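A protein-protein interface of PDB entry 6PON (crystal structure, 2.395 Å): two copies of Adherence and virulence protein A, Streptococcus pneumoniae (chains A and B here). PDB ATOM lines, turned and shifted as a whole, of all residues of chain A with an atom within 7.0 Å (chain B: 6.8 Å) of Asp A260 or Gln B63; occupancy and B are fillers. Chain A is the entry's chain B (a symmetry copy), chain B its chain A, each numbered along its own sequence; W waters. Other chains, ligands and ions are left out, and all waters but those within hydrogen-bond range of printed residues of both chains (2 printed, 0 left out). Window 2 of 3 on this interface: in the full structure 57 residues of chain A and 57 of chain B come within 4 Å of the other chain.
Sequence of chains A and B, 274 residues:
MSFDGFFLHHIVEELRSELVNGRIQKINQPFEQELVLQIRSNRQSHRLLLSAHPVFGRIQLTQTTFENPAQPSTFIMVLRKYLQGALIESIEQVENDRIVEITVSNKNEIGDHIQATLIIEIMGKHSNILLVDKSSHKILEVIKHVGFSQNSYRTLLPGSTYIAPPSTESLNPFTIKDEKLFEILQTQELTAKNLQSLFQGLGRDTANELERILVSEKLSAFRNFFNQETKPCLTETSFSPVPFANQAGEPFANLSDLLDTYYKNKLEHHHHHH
The backbone carbonyl oxygen of Leu B61 lies close to the side-chain hydroxyl of Ser A256 (3.2 Å). The backbone NH (N) of Gln B63 is in hydrogen-bond range of the side-chain carboxylate (OD2) of Asp A260. The side-chain amide nitrogen (NE2) of Gln B60 sits at hydrogen-bond distance from the side-chain carboxylate (OD1) of Asp A260 (2.9 Å). The side-chain hydroxyl of Thr B62 is in hydrogen-bond range of the side-chain carboxylate of Asp A260.
The backbone carbonyl oxygen (O) of Arg B47 lies within hydrogen-bond range of the backbone NH (N) of Thr B62. O of Gln B60 lies within hydrogen-bond range of N of Leu B49, at 2.7 Å. OD1 of Asn A254 sits close to N of Ser A256, at 3.5 Å. The side-chain hydroxyl (OG1) of Thr B62 is in hydrogen-bond range of the backbone NH (N) of Thr B64 (3.2 Å). OE1 of Gln B60 is in hydrogen-bond range of NE of Arg B58 (3.0 Å).
Among the printed residues, merely in contact across the chains: Tyr A263 with Arg B58 (3.4 Å), Leu A259 with Gln B60 (3.4 Å), Ser A256 with Gln B60 (3.6 Å) and Ser A256 with Thr B62 (3.8 Å).
Of the printed residues of chain B, Ser A256 touches Gln B60 (3.6 Å), Leu B61 (3.1 Å) and Thr B62 (3.8 Å). Of chain B, only Gln B60, Thr B62 and Gln B63 come within 4 Å of Asp A260. Tyr A262 touches none of the printed residues of chain B. Printed residues of chain A within 4 Å of Leu B61: Ser A256. Printed residues of chain A within 4 Å of Thr B62: Ser A256 and Asp A260. Gln B63 touches one residue of chain A. The nearest residue of chain B that does not touch Asp A260 is Thr B64 (4.1 Å). The nearest residue of chain A that does not touch Gln B63 is Ser A256 (4.4 Å). The nearest printed residue of chain B that does not touch Leu A259 is Arg B58 (4.9 Å).
Of the 12 printed residues of chain A, 4 touch a printed residue of chain B. Hydrophobic or aromatic side chains of chain B within 4 Å of the printed part of chain A: Leu B61. Among the printed residues, no Asp or Glu carboxylate lies within 4 Å of a Lys or Arg side-chain nitrogen of the other chain.
No position is printed for both chains. Of the 8 pairs that touch across the chains among the printed residues, none has its exchanged pair printed and touching as well.
Water W2 lies within hydrogen-bond range of OE1 of Gln B63 (2.8 Å) and OG of Ser A256 (3.0 Å). Water W1 lies within hydrogen-bond range of the backbone NH of Leu B61 (3.0 Å) and the backbone NH of Ser A256 (3.4 Å).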
ATOM      1  N   ASN A 254     -26.769  -0.858   3.345  1.00  0.00           N
ATOM      2  CA  ASN A 254     -26.095   0.412   3.132  1.00  0.00           C
ATOM      3  C   ASN A 254     -26.276   0.827   1.684  1.00  0.00           C
ATOM      4  O   ASN A 254     -26.766   0.065   0.850  1.00  0.00           O
ATOM      5  CB  ASN A 254     -24.622   0.304   3.490  1.00  0.00           C
ATOM      6  CG  ASN A 254     -24.037  -0.974   2.998  1.00  0.00           C
ATOM      7  OD1 ASN A 254     -23.889  -1.175   1.788  1.00  0.00           O
ATOM      8  ND2 ASN A 254     -23.739  -1.875   3.914  1.00  0.00           N
ATOM      9  N   LEU A 255     -25.850   2.047   1.395  1.00  0.00           N
ATOM     10  CA  LEU A 255     -26.073   2.610   0.078  1.00  0.00           C
ATOM     11  C   LEU A 255     -25.203   1.944  -0.976  1.00  0.00           C
ATOM     12  O   LEU A 255     -25.573   1.944  -2.153  1.00  0.00           O
ATOM     13  CB  LEU A 255     -25.829   4.119   0.132  1.00  0.00           C
ATOM     14  CG  LEU A 255     -26.647   4.806   1.233  1.00  0.00           C
ATOM     15  CD1 LEU A 255     -25.994   6.093   1.739  1.00  0.00           C
ATOM     16  CD2 LEU A 255     -28.054   5.070   0.748  1.00  0.00           C
ATOM     17  N   SER A 256     -24.079   1.351  -0.572  1.00  0.00           N
ATOM     18  CA  SER A 256     -23.224   0.633  -1.505  1.00  0.00           C
ATOM     19  C   SER A 256     -23.936  -0.583  -2.077  1.00  0.00           C
ATOM     20  O   SER A 256     -23.941  -0.798  -3.293  1.00  0.00           O
ATOM     21  CB  SER A 256     -21.926   0.213  -0.801  1.00  0.00           C
ATOM     22  OG  SER A 256     -21.425  -1.034  -1.304  1.00  0.00           O
ATOM     23  N   ASP A 257     -24.536  -1.401  -1.209  1.00  0.00           N
ATOM     24  CA  ASP A 257     -25.273  -2.570  -1.669  1.00  0.00           C
ATOM     25  C   ASP A 257     -26.457  -2.165  -2.532  1.00  0.00           C
ATOM     26  O   ASP A 257     -26.779  -2.841  -3.517  1.00  0.00           O
ATOM     27  CB  ASP A 257     -25.768  -3.391  -0.475  1.00  0.00           C
ATOM     28  CG  ASP A 257     -24.649  -4.022   0.339  1.00  0.00           C
ATOM     29  OD1 ASP A 257     -23.446  -3.761   0.081  1.00  0.00           O
ATOM     30  OD2 ASP A 257     -24.994  -4.778   1.273  1.00  0.00           O
ATOM     31  N   LEU A 258     -27.147  -1.088  -2.151  1.00  0.00           N
ATOM     32  CA  LEU A 258     -28.277  -0.606  -2.947  1.00  0.00           C
ATOM     33  C   LEU A 258     -27.827  -0.238  -4.363  1.00  0.00           C
ATOM     34  O   LEU A 258     -28.427  -0.670  -5.359  1.00  0.00           O
ATOM     35  CB  LEU A 258     -28.938   0.588  -2.240  1.00  0.00           C
ATOM     36  CG  LEU A 258     -29.895   1.456  -3.068  1.00  0.00           C
ATOM     37  CD1 LEU A 258     -31.096   0.647  -3.489  1.00  0.00           C
ATOM     38  CD2 LEU A 258     -30.365   2.703  -2.302  1.00  0.00           C
ATOM     39  N   LEU A 259     -26.739   0.527  -4.474  1.00  0.00           N
ATOM     40  CA  LEU A 259     -26.289   1.005  -5.778  1.00  0.00           C
ATOM     41  C   LEU A 259     -25.608  -0.097  -6.598  1.00  0.00           C
ATOM     42  O   LEU A 259     -25.841  -0.192  -7.806  1.00  0.00           O
ATOM     43  CB  LEU A 259     -25.369   2.206  -5.575  1.00  0.00           C
ATOM     44  CG  LEU A 259     -26.103   3.434  -5.048  1.00  0.00           C
ATOM     45  CD1 LEU A 259     -25.153   4.590  -4.880  1.00  0.00           C
ATOM     46  CD2 LEU A 259     -27.245   3.813  -5.997  1.00  0.00           C
ATOM     47  N   ASP A 260     -24.793  -0.953  -5.965  1.00  0.00           N
ATOM     48  CA  ASP A 260     -24.245  -2.121  -6.669  1.00  0.00           C
ATOM     49  C   ASP A 260     -25.362  -2.908  -7.340  1.00  0.00           C
ATOM     50  O   ASP A 260     -25.249  -3.307  -8.506  1.00  0.00           O
ATOM     51  CB  ASP A 260     -23.477  -3.047  -5.712  1.00  0.00           C
ATOM     52  CG  ASP A 260     -22.092  -2.515  -5.328  1.00  0.00           C
ATOM     53  OD1 ASP A 260     -21.663  -1.472  -5.876  1.00  0.00           O
ATOM     54  OD2 ASP A 260     -21.422  -3.148  -4.482  1.00  0.00           O
ATOM     55  N   THR A 261     -26.473  -3.091  -6.619  1.00  0.00           N
ATOM     56  CA  THR A 261     -27.598  -3.854  -7.136  1.00  0.00           C
ATOM     57  C   THR A 261     -28.329  -3.084  -8.229  1.00  0.00           C
ATOM     58  O   THR A 261     -28.695  -3.655  -9.264  1.00  0.00           O
ATOM     59  CB  THR A 261     -28.551  -4.198  -5.986  1.00  0.00           C
ATOM     60  OG1 THR A 261     -27.854  -4.974  -5.008  1.00  0.00           O
ATOM     61  CG2 THR A 261     -29.777  -4.954  -6.492  1.00  0.00           C
ATOM     62  N   TYR A 262     -28.564  -1.790  -8.014  1.00  0.00           N
ATOM     63  CA  TYR A 262     -29.260  -1.019  -9.034  1.00  0.00           C
ATOM     64  C   TYR A 262     -28.491  -1.005 -10.350  1.00  0.00           C
ATOM     65  O   TYR A 262     -29.089  -1.129 -11.423  1.00  0.00           O
ATOM     66  CB  TYR A 262     -29.496   0.399  -8.544  1.00  0.00           C
ATOM     67  CG  TYR A 262     -30.206   1.252  -9.535  1.00  0.00           C
ATOM     68  CD1 TYR A 262     -31.582   1.154  -9.691  1.00  0.00           C
ATOM     69  CD2 TYR A 262     -29.507   2.164 -10.327  1.00  0.00           C
ATOM     70  CE1 TYR A 262     -32.261   1.932 -10.602  1.00  0.00           C
ATOM     71  CE2 TYR A 262     -30.182   2.957 -11.264  1.00  0.00           C
ATOM     72  CZ  TYR A 262     -31.564   2.831 -11.387  1.00  0.00           C
ATOM     73  OH  TYR A 262     -32.260   3.605 -12.275  1.00  0.00           O
ATOM     74  N   TYR A 263     -27.169  -0.853 -10.295  1.00  0.00           N
ATOM     75  CA  TYR A 263     -26.384  -0.599 -11.501  1.00  0.00           C
ATOM     76  C   TYR A 263     -25.777  -1.855 -12.096  1.00  0.00           C
ATOM     77  O   TYR A 263     -25.113  -1.759 -13.136  1.00  0.00           O
ATOM     78  CB  TYR A 263     -25.266   0.423 -11.213  1.00  0.00           C
ATOM     79  CG  TYR A 263     -25.788   1.835 -11.126  1.00  0.00           C
ATOM     80  CD1 TYR A 263     -26.259   2.492 -12.254  1.00  0.00           C
ATOM     81  CD2 TYR A 263     -25.833   2.501  -9.925  1.00  0.00           C
ATOM     82  CE1 TYR A 263     -26.743   3.773 -12.182  1.00  0.00           C
ATOM     83  CE2 TYR A 263     -26.344   3.770  -9.841  1.00  0.00           C
ATOM     84  CZ  TYR A 263     -26.791   4.410 -10.972  1.00  0.00           C
ATOM     85  OH  TYR A 263     -27.299   5.691 -10.877  1.00  0.00           O
ATOM     86  N   LYS A 264     -26.002  -3.017 -11.472  1.00  0.00           N
ATOM     87  CA  LYS A 264     -25.236  -4.219 -11.781  1.00  0.00           C
ATOM     88  C   LYS A 264     -25.258  -4.538 -13.274  1.00  0.00           C
ATOM     89  O   LYS A 264     -24.212  -4.662 -13.923  1.00  0.00           O
ATOM     90  CB  LYS A 264     -25.771  -5.404 -10.974  1.00  0.00           C
ATOM     91  CG  LYS A 264     -24.835  -6.606 -11.012  1.00  0.00           C
ATOM     92  CD  LYS A 264     -25.577  -7.921 -11.086  1.00  0.00           C
ATOM     93  CE  LYS A 264     -25.739  -8.551  -9.717  1.00  0.00           C
ATOM     94  NZ  LYS A 264     -26.035 -10.024  -9.793  1.00  0.00           N
ATOM     95  N   ASN A 265     -26.442  -4.681 -13.843  1.00  0.00           N
ATOM     96  CA  ASN A 265     -26.528  -5.081 -15.241  1.00  0.00           C
ATOM     97  C   ASN A 265     -26.953  -3.926 -16.132  1.00  0.00           C
ATOM     98  O   ASN A 265     -27.574  -4.130 -17.173  1.00  0.00           O
ATOM     99  CB  ASN A 265     -27.482  -6.265 -15.399  1.00  0.00           C
ATOM    100  CG  ASN A 265     -27.346  -7.274 -14.272  1.00  0.00           C
ATOM    101  OD1 ASN A 265     -27.977  -7.128 -13.225  1.00  0.00           O
ATOM    102  ND2 ASN A 265     -26.498  -8.290 -14.470  1.00  0.00           N
ATOM    103  N   GLN B  44     -10.017  -2.363   8.119  1.00  0.00           N
ATOM    104  CA  GLN B  44     -10.831  -2.917   7.047  1.00  0.00           C
ATOM    105  C   GLN B  44     -10.502  -2.222   5.732  1.00  0.00           C
ATOM    106  O   GLN B  44     -10.103  -1.054   5.702  1.00  0.00           O
ATOM    107  CB  GLN B  44     -12.325  -2.801   7.358  1.00  0.00           C
ATOM    108  CG  GLN B  44     -13.223  -3.431   6.308  1.00  0.00           C
ATOM    109  CD  GLN B  44     -14.619  -3.707   6.824  1.00  0.00           C
ATOM    110  OE1 GLN B  44     -14.806  -4.006   8.009  1.00  0.00           O
ATOM    111  NE2 GLN B  44     -15.616  -3.587   5.939  1.00  0.00           N
ATOM    112  N   SER B  45     -10.647  -2.959   4.649  1.00  0.00           N
ATOM    113  CA  SER B  45     -10.401  -2.454   3.312  1.00  0.00           C
ATOM    114  C   SER B  45     -11.714  -1.993   2.680  1.00  0.00           C
ATOM    115  O   SER B  45     -12.774  -2.560   2.938  1.00  0.00           O
ATOM    116  CB  SER B  45      -9.746  -3.546   2.466  1.00  0.00           C
ATOM    117  OG  SER B  45      -9.643  -3.153   1.113  1.00  0.00           O
ATOM    118  N   ARG B  47     -13.478  -0.240  -1.126  1.00  0.00           N
ATOM    119  CA  ARG B  47     -13.337   0.113  -2.535  1.00  0.00           C
ATOM    120  C   ARG B  47     -14.293   1.259  -2.855  1.00  0.00           C
ATOM    121  O   ARG B  47     -15.509   1.115  -2.713  1.00  0.00           O
ATOM    122  CB  ARG B  47     -13.608  -1.103  -3.428  1.00  0.00           C
ATOM    123  CG  ARG B  47     -13.206  -0.900  -4.873  1.00  0.00           C
ATOM    124  CD  ARG B  47     -13.145  -2.227  -5.582  1.00  0.00           C
ATOM    125  NE  ARG B  47     -12.265  -3.130  -4.852  1.00  0.00           N
ATOM    126  CZ  ARG B  47     -12.314  -4.456  -4.939  1.00  0.00           C
ATOM    127  NH1 ARG B  47     -13.216  -5.038  -5.718  1.00  0.00           N
ATOM    128  NH2 ARG B  47     -11.471  -5.200  -4.229  1.00  0.00           N
ATOM    129  N   LEU B  49     -15.758   3.971  -5.589  1.00  0.00           N
ATOM    130  CA  LEU B  49     -15.982   4.298  -6.989  1.00  0.00           C
ATOM    131  C   LEU B  49     -16.345   5.774  -7.126  1.00  0.00           C
ATOM    132  O   LEU B  49     -17.241   6.268  -6.432  1.00  0.00           O
ATOM    133  CB  LEU B  49     -17.098   3.427  -7.573  1.00  0.00           C
ATOM    134  CG  LEU B  49     -17.569   3.751  -8.999  1.00  0.00           C
ATOM    135  CD1 LEU B  49     -16.447   3.469  -9.985  1.00  0.00           C
ATOM    136  CD2 LEU B  49     -18.831   2.970  -9.358  1.00  0.00           C
ATOM    137  N   ARG B  58     -21.829   9.011 -10.391  1.00  0.00           N
ATOM    138  CA  ARG B  58     -22.134   8.782  -8.988  1.00  0.00           C
ATOM    139  C   ARG B  58     -20.816   8.630  -8.249  1.00  0.00           C
ATOM    140  O   ARG B  58     -19.742   8.560  -8.863  1.00  0.00           O
ATOM    141  CB  ARG B  58     -22.989   7.533  -8.798  1.00  0.00           C
ATOM    142  CG  ARG B  58     -22.275   6.230  -9.218  1.00  0.00           C
ATOM    143  CD  ARG B  58     -23.280   5.097  -9.368  1.00  0.00           C
ATOM    144  NE  ARG B  58     -22.706   3.783  -9.686  1.00  0.00           N
ATOM    145  CZ  ARG B  58     -22.298   3.400 -10.899  1.00  0.00           C
ATOM    146  NH1 ARG B  58     -22.357   4.238 -11.917  1.00  0.00           N
ATOM    147  NH2 ARG B  58     -21.820   2.181 -11.101  1.00  0.00           N
ATOM    148  N   GLN B  60     -19.654   6.141  -4.688  1.00  0.00           N
ATOM    149  CA  GLN B  60     -20.182   5.099  -3.819  1.00  0.00           C
ATOM    150  C   GLN B  60     -19.048   4.162  -3.419  1.00  0.00           C
ATOM    151  O   GLN B  60     -18.075   3.996  -4.157  1.00  0.00           O
ATOM    152  CB  GLN B  60     -21.303   4.307  -4.514  1.00  0.00           C
ATOM    153  CG  GLN B  60     -20.855   3.569  -5.778  1.00  0.00           C
ATOM    154  CD  GLN B  60     -21.727   2.335  -6.117  1.00  0.00           C
ATOM    155  OE1 GLN B  60     -22.356   2.272  -7.173  1.00  0.00           O
ATOM    156  NE2 GLN B  60     -21.740   1.349  -5.217  1.00  0.00           N
ATOM    157  N   LEU B  61     -19.168   3.584  -2.226  1.00  0.00           N
ATOM    158  CA  LEU B  61     -18.411   2.385  -1.906  1.00  0.00           C
ATOM    159  C   LEU B  61     -18.981   1.252  -2.747  1.00  0.00           C
ATOM    160  O   LEU B  61     -20.150   1.284  -3.153  1.00  0.00           O
ATOM    161  CB  LEU B  61     -18.503   2.064  -0.408  1.00  0.00           C
ATOM    162  CG  LEU B  61     -17.937   3.115   0.552  1.00  0.00           C
ATOM    163  CD1 LEU B  61     -18.574   3.050   1.923  1.00  0.00           C
ATOM    164  CD2 LEU B  61     -16.435   2.933   0.677  1.00  0.00           C
ATOM    165  N   THR B  62     -18.151   0.262  -3.050  1.00  0.00           N
ATOM    166  CA  THR B  62     -18.648  -0.770  -3.940  1.00  0.00           C
ATOM    167  C   THR B  62     -17.973  -2.095  -3.632  1.00  0.00           C
ATOM    168  O   THR B  62     -16.868  -2.146  -3.073  1.00  0.00           O
ATOM    169  CB  THR B  62     -18.445  -0.397  -5.413  1.00  0.00           C
ATOM    170  OG1 THR B  62     -19.086  -1.374  -6.226  1.00  0.00           O
ATOM    171  CG2 THR B  62     -16.961  -0.349  -5.773  1.00  0.00           C
ATOM    172  N   GLN B  63     -18.690  -3.169  -3.983  1.00  0.00           N
ATOM    173  CA  GLN B  63     -18.194  -4.535  -3.899  1.00  0.00           C
ATOM    174  C   GLN B  63     -17.771  -5.095  -5.247  1.00  0.00           C
ATOM    175  O   GLN B  63     -17.248  -6.205  -5.296  1.00  0.00           O
ATOM    176  CB  GLN B  63     -19.265  -5.449  -3.305  1.00  0.00           C
ATOM    177  CG  GLN B  63     -19.566  -5.176  -1.855  1.00  0.00           C
ATOM    178  CD  GLN B  63     -18.428  -5.586  -0.979  1.00  0.00           C
ATOM    179  OE1 GLN B  63     -17.934  -4.796  -0.165  1.00  0.00           O
ATOM    180  NE2 GLN B  63     -17.980  -6.830  -1.144  1.00  0.00           N
ATOM    181  N   THR B  64     -18.010  -4.365  -6.329  1.00  0.00           N
ATOM    182  CA  THR B  64     -17.690  -4.847  -7.660  1.00  0.00           C
ATOM    183  C   THR B  64     -16.189  -5.040  -7.810  1.00  0.00           C
ATOM    184  O   THR B  64     -15.395  -4.216  -7.357  1.00  0.00           O
ATOM    185  CB  THR B  64     -18.196  -3.841  -8.695  1.00  0.00           C
ATOM    186  OG1 THR B  64     -19.626  -3.801  -8.664  1.00  0.00           O
ATOM    187  CG2 THR B  64     -17.690  -4.183 -10.109  1.00  0.00           C
ATOM    188  N   THR B  65     -15.797  -6.140  -8.433  1.00  0.00           N
ATOM    189  CA  THR B  65     -14.416  -6.292  -8.867  1.00  0.00           C
ATOM    190  C   THR B  65     -14.282  -5.695 -10.254  1.00  0.00           C
ATOM    191  O   THR B  65     -15.174  -5.855 -11.088  1.00  0.00           O
ATOM    192  CB  THR B  65     -13.988  -7.755  -8.886  1.00  0.00           C
ATOM    193  OG1 THR B  65     -14.223  -8.318  -7.594  1.00  0.00           O
ATOM    194  CG2 THR B  65     -12.501  -7.839  -9.199  1.00  0.00           C
ATOM    195  N   PHE B  66     -13.190  -4.976 -10.485  1.00  0.00           N
ATOM    196  CA  PHE B  66     -12.968  -4.312 -11.761  1.00  0.00           C
ATOM    197  C   PHE B  66     -11.775  -4.915 -12.492  1.00  0.00           C
ATOM    198  O   PHE B  66     -10.797  -5.349 -11.874  1.00  0.00           O
ATOM    199  CB  PHE B  66     -12.733  -2.812 -11.562  1.00  0.00           C
ATOM    200  CG  PHE B  66     -13.959  -2.053 -11.127  1.00  0.00           C
ATOM    201  CD1 PHE B  66     -14.257  -1.904  -9.775  1.00  0.00           C
ATOM    202  CD2 PHE B  66     -14.811  -1.481 -12.071  1.00  0.00           C
ATOM    203  CE1 PHE B  66     -15.395  -1.197  -9.367  1.00  0.00           C
ATOM    204  CE2 PHE B  66     -15.945  -0.773 -11.679  1.00  0.00           C
ATOM    205  CZ  PHE B  66     -16.239  -0.628 -10.321  1.00  0.00           C
HETATM  206  O   HOH W   1     -21.545   3.576  -0.340  1.00  0.00           O
HETATM  207  O   HOH W   2     -18.924  -2.196  -0.093  1.00  0.00           O
